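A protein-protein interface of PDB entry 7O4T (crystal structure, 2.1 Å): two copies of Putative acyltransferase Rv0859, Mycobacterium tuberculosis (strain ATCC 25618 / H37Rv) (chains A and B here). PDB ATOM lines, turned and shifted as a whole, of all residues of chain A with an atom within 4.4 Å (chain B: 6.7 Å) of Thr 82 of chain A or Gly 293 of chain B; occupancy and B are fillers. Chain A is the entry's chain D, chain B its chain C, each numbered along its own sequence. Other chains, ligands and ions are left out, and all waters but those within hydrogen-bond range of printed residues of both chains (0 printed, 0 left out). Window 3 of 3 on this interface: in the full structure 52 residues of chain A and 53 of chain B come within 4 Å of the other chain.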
ATOM      1  N   ILE A  51      33.621  -2.639   4.459  1.00  0.00           N
ATOM      2  CA  ILE A  51      33.611  -3.928   3.775  1.00  0.00           C
ATOM      3  C   ILE A  51      32.707  -3.811   2.555  1.00  0.00           C
ATOM      4  O   ILE A  51      31.505  -3.556   2.684  1.00  0.00           O
ATOM      5  CB  ILE A  51      33.138  -5.051   4.709  1.00  0.00           C
ATOM      6  CG1 ILE A  51      34.096  -5.202   5.892  1.00  0.00           C
ATOM      7  CG2 ILE A  51      33.009  -6.358   3.943  1.00  0.00           C
ATOM      8  CD1 ILE A  51      33.663  -6.256   6.889  1.00  0.00           C
ATOM      9  N   SER A  52      33.282  -4.000   1.369  1.00  0.00           N
ATOM     10  CA  SER A  52      32.562  -3.753   0.128  1.00  0.00           C
ATOM     11  C   SER A  52      32.055  -5.017  -0.554  1.00  0.00           C
ATOM     12  O   SER A  52      31.233  -4.909  -1.471  1.00  0.00           O
ATOM     13  CB  SER A  52      33.445  -2.964  -0.850  1.00  0.00           C
ATOM     14  OG  SER A  52      34.674  -3.628  -1.088  1.00  0.00           O
ATOM     15  N   PRO A  80      26.331  -4.473   7.169  1.00  0.00           N
ATOM     16  CA  PRO A  80      25.756  -3.373   6.386  1.00  0.00           C
ATOM     17  C   PRO A  80      25.222  -3.869   5.052  1.00  0.00           C
ATOM     18  O   PRO A  80      25.836  -4.704   4.384  1.00  0.00           O
ATOM     19  CB  PRO A  80      26.936  -2.413   6.200  1.00  0.00           C
ATOM     20  CG  PRO A  80      27.812  -2.677   7.372  1.00  0.00           C
ATOM     21  CD  PRO A  80      27.689  -4.154   7.643  1.00  0.00           C
ATOM     22  N   VAL A  81      24.057  -3.343   4.671  1.00  0.00           N
ATOM     23  CA  VAL A  81      23.405  -3.773   3.443  1.00  0.00           C
ATOM     24  C   VAL A  81      24.199  -3.410   2.197  1.00  0.00           C
ATOM     25  O   VAL A  81      23.884  -3.900   1.106  1.00  0.00           O
ATOM     26  CB  VAL A  81      21.983  -3.177   3.395  1.00  0.00           C
ATOM     27  CG1 VAL A  81      22.009  -1.780   2.797  1.00  0.00           C
ATOM     28  CG2 VAL A  81      21.048  -4.100   2.648  1.00  0.00           C
ATOM     29  N   THR A  82      25.231  -2.579   2.332  1.00  0.00           N
ATOM     30  CA  THR A  82      26.121  -2.233   1.233  1.00  0.00           C
ATOM     31  C   THR A  82      27.304  -3.186   1.097  1.00  0.00           C
ATOM     32  O   THR A  82      28.179  -2.944   0.260  1.00  0.00           O
ATOM     33  CB  THR A  82      26.646  -0.803   1.409  1.00  0.00           C
ATOM     34  OG1 THR A  82      27.429  -0.725   2.606  1.00  0.00           O
ATOM     35  CG2 THR A  82      25.491   0.180   1.504  1.00  0.00           C
ATOM     36  N   SER A  83      27.353  -4.259   1.887  1.00  0.00           N
ATOM     37  CA  SER A  83      28.494  -5.168   1.891  1.00  0.00           C
ATOM     38  C   SER A  83      28.425  -6.234   0.802  1.00  0.00           C
ATOM     39  O   SER A  83      29.276  -7.129   0.787  1.00  0.00           O
ATOM     40  CB  SER A  83      28.628  -5.838   3.261  1.00  0.00           C
ATOM     41  OG  SER A  83      29.027  -4.899   4.244  1.00  0.00           O
ATOM     42  N   GLY A  84      27.442  -6.172  -0.091  1.00  0.00           N
ATOM     43  CA  GLY A  84      27.445  -7.061  -1.243  1.00  0.00           C
ATOM     44  C   GLY A  84      27.135  -8.499  -0.873  1.00  0.00           C
ATOM     45  O   GLY A  84      26.270  -8.785  -0.037  1.00  0.00           O
ATOM     46  N   THR B 291      30.281  -1.423  -6.374  1.00  0.00           N
ATOM     47  CA  THR B 291      29.185  -2.188  -5.801  1.00  0.00           C
ATOM     48  C   THR B 291      28.753  -1.528  -4.501  1.00  0.00           C
ATOM     49  O   THR B 291      29.592  -1.125  -3.690  1.00  0.00           O
ATOM     50  CB  THR B 291      29.583  -3.646  -5.532  1.00  0.00           C
ATOM     51  OG1 THR B 291      30.544  -3.691  -4.471  1.00  0.00           O
ATOM     52  CG2 THR B 291      30.187  -4.278  -6.777  1.00  0.00           C
ATOM     53  N   SER B 292      27.441  -1.413  -4.312  1.00  0.00           N
ATOM     54  CA  SER B 292      26.898  -0.862  -3.077  1.00  0.00           C
ATOM     55  C   SER B 292      25.577  -1.545  -2.751  1.00  0.00           C
ATOM     56  O   SER B 292      25.358  -2.697  -3.142  1.00  0.00           O
ATOM     57  CB  SER B 292      26.717   0.652  -3.193  1.00  0.00           C
ATOM     58  OG  SER B 292      26.456   1.228  -1.925  1.00  0.00           O
ATOM     59  N   GLY B 293      24.689  -0.856  -2.045  1.00  0.00           N
ATOM     60  CA  GLY B 293      23.415  -1.461  -1.703  1.00  0.00           C
ATOM     61  C   GLY B 293      22.511  -0.492  -0.974  1.00  0.00           C
ATOM     62  O   GLY B 293      22.894   0.637  -0.648  1.00  0.00           O
ATOM     63  N   ALA B 294      21.289  -0.962  -0.731  1.00  0.00           N
ATOM     64  CA  ALA B 294      20.286  -0.233   0.031  1.00  0.00           C
ATOM     65  C   ALA B 294      19.345  -1.255   0.659  1.00  0.00           C
ATOM     66  O   ALA B 294      19.526  -2.466   0.504  1.00  0.00           O
ATOM     67  CB  ALA B 294      19.537   0.770  -0.850  1.00  0.00           C
ATOM     68  N   ASP B 295      18.325  -0.753   1.368  1.00  0.00           N
ATOM     69  CA  ASP B 295      17.377  -1.550   2.145  1.00  0.00           C
ATOM     70  C   ASP B 295      16.911  -2.795   1.394  1.00  0.00           C
ATOM     71  O   ASP B 295      16.482  -2.700   0.237  1.00  0.00           O
ATOM     72  CB  ASP B 295      16.169  -0.698   2.537  1.00  0.00           C
ATOM     73  CG  ASP B 295      15.093  -1.500   3.243  1.00  0.00           C
ATOM     74  OD1 ASP B 295      15.357  -1.999   4.358  1.00  0.00           O
ATOM     75  OD2 ASP B 295      13.984  -1.634   2.685  1.00  0.00           O
ATOM     76  N   THR B 301      16.408  -0.258  -4.661  1.00  0.00           N
ATOM     77  CA  THR B 301      16.987   1.081  -4.658  1.00  0.00           C
ATOM     78  C   THR B 301      18.511   1.053  -4.633  1.00  0.00           C
ATOM     79  O   THR B 301      19.141   2.089  -4.393  1.00  0.00           O
ATOM     80  CB  THR B 301      16.455   1.897  -3.479  1.00  0.00           C
ATOM     81  OG1 THR B 301      16.671   1.181  -2.257  1.00  0.00           O
ATOM     82  CG2 THR B 301      14.967   2.169  -3.653  1.00  0.00           C
ATOM     83  N   GLY B 302      19.112  -0.108  -4.876  1.00  0.00           N
ATOM     84  CA  GLY B 302      20.547  -0.248  -4.969  1.00  0.00           C
ATOM     85  C   GLY B 302      21.244   0.535  -6.075  1.00  0.00           C
ATOM     86  O   GLY B 302      22.390   0.960  -5.900  1.00  0.00           O
ATOM     87  N   PRO B 303      20.601   0.710  -7.246  1.00  0.00           N
ATOM     88  CA  PRO B 303      21.263   1.469  -8.327  1.00  0.00           C
ATOM     89  C   PRO B 303      21.755   2.859  -7.946  1.00  0.00           C
ATOM     90  O   PRO B 303      22.807   3.279  -8.444  1.00  0.00           O
ATOM     91  CB  PRO B 303      20.172   1.544  -9.402  1.00  0.00           C
ATOM     92  CG  PRO B 303      19.432   0.291  -9.241  1.00  0.00           C
ATOM     93  CD  PRO B 303      19.421  -0.011  -7.764  1.00  0.00           C
ATOM     94  N   PRO B 305      22.957   4.398  -4.929  1.00  0.00           N
ATOM     95  CA  PRO B 305      24.270   4.516  -4.269  1.00  0.00           C
ATOM     96  C   PRO B 305      25.410   3.927  -5.081  1.00  0.00           C
ATOM     97  O   PRO B 305      26.533   4.438  -5.009  1.00  0.00           O
ATOM     98  CB  PRO B 305      24.071   3.764  -2.946  1.00  0.00           C
ATOM     99  CG  PRO B 305      22.959   2.819  -3.215  1.00  0.00           C
ATOM    100  CD  PRO B 305      22.038   3.554  -4.142  1.00  0.00           C
ATOM    101  N   ALA B 306      25.159   2.867  -5.853  1.00  0.00           N
ATOM    102  CA  ALA B 306      26.223   2.277  -6.660  1.00  0.00           C
ATOM    103  C   ALA B 306      26.620   3.196  -7.808  1.00  0.00           C
ATOM    104  O   ALA B 306      27.802   3.281  -8.163  1.00  0.00           O
ATOM    105  CB  ALA B 306      25.786   0.912  -7.188  1.00  0.00           C
ATOM    106  N   LYS B 309      28.623   5.962  -6.364  1.00  0.00           N
ATOM    107  CA  LYS B 309      29.950   5.515  -5.955  1.00  0.00           C
ATOM    108  C   LYS B 309      30.884   5.367  -7.150  1.00  0.00           C
ATOM    109  O   LYS B 309      32.077   5.673  -7.050  1.00  0.00           O
ATOM    110  CB  LYS B 309      29.830   4.197  -5.189  1.00  0.00           C
ATOM    111  CG  LYS B 309      31.123   3.667  -4.588  1.00  0.00           C
ATOM    112  CD  LYS B 309      30.845   2.408  -3.773  1.00  0.00           C
ATOM    113  CE  LYS B 309      32.123   1.751  -3.285  1.00  0.00           C
ATOM    114  NZ  LYS B 309      31.855   0.503  -2.514  1.00  0.00           N
ATOM    115  N   GLY B 393      18.760  -6.122  -2.120  1.00  0.00           N
ATOM    116  CA  GLY B 393      19.090  -4.731  -1.892  1.00  0.00           C
ATOM    117  C   GLY B 393      20.462  -4.301  -2.355  1.00  0.00           C
ATOM    118  O   GLY B 393      20.988  -3.311  -1.834  1.00  0.00           O
ATOM    119  N   MET B 394      21.059  -5.003  -3.315  1.00  0.00           N
ATOM    120  CA  MET B 394      22.390  -4.670  -3.800  1.00  0.00           C
ATOM    121  C   MET B 394      22.309  -3.796  -5.051  1.00  0.00           C
ATOM    122  O   MET B 394      21.239  -3.567  -5.621  1.00  0.00           O
ATOM    123  CB  MET B 394      23.185  -5.943  -4.094  1.00  0.00           C
ATOM    124  CG  MET B 394      23.484  -6.798  -2.881  1.00  0.00           C
ATOM    125  SD  MET B 394      24.493  -8.247  -3.259  1.00  0.00           S
ATOM    126  CE  MET B 394      23.269  -9.368  -3.934  1.00  0.00           C
ATOM    127  N   GLY B 395      23.471  -3.301  -5.475  1.00  0.00           N
ATOM    128  CA  GLY B 395      23.582  -2.487  -6.671  1.00  0.00           C
ATOM    129  C   GLY B 395      24.968  -2.551  -7.281  1.00  0.00           C
ATOM    130  O   GLY B 395      25.966  -2.532  -6.556  1.00  0.00           O
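OG1 of Thr 291 of chain B sits at hydrogen-bond distance from O of Ser 52 of chain A (3.3 Å). O of Gly 84 of chain A lies close to SD of Met 394 of chain B, 3.7 Å away.
O of Val 81 of chain A touches CA of Gly 293 of chain B, at 3.7 Å. Ala 294 of chain B touches Val 81 of chain A. CG2 of Thr 82 of chain A touches OG of Ser 292 of chain B, 3.7 Å away. Thr 82 of chain A touches Gly 293 of chain B.
No position is printed for both chains. Of the 6 pairs that touch across the chains among the printed residues, none has its exchanged pair printed and touching as well.
Thr 82 of chain A touches two residues of chain B. Of chain A, only Val 81 and Thr 82 come within 4 Å of Gly 293 of chain B. Of the printed residues of chain B, Gly 84 of chain A touches Met 394. Of the printed residues of chain A, Ala 294 of chain B touches Val 81. Ala 306 of chain B touches none of the printed residues of chain A. The nearest residue of chain B that does not touch Thr 82 of chain A is Thr 291 of chain B (4.6 Å). The nearest printed residue of chain A that does not touch Gly 293 of chain B is Ser 83 of chain A (5.8 Å). The nearest printed residue of chain B that does not touch Gly 84 of chain A is Ser 292 of chain B (5.1 Å).
The side-chain amino group (NZ) of Lys 309 of chain B lies within hydrogen-bond range of the backbone carbonyl oxygen (O) of Thr 291 of chain B (3.0 Å). N of Ser 292 of chain B lies within hydrogen-bond range of O of Gly 395 of chain B (2.9 Å). The backbone NH of Ala 294 of chain B sits at hydrogen-bond distance from the backbone carbonyl oxygen of Gly 393 of chain B (2.6 Å).
Of the 14 printed residues of chain B, 5 touch a printed residue of chain A. Hydrophobic or aromatic side chains of chain B within 4 Å of the printed part of chain A: Met 394. Along chain B the printed residues that touch a printed residue of chain A span positions 291 to 394. Among the printed residues, 6 pairs touch across the chains.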
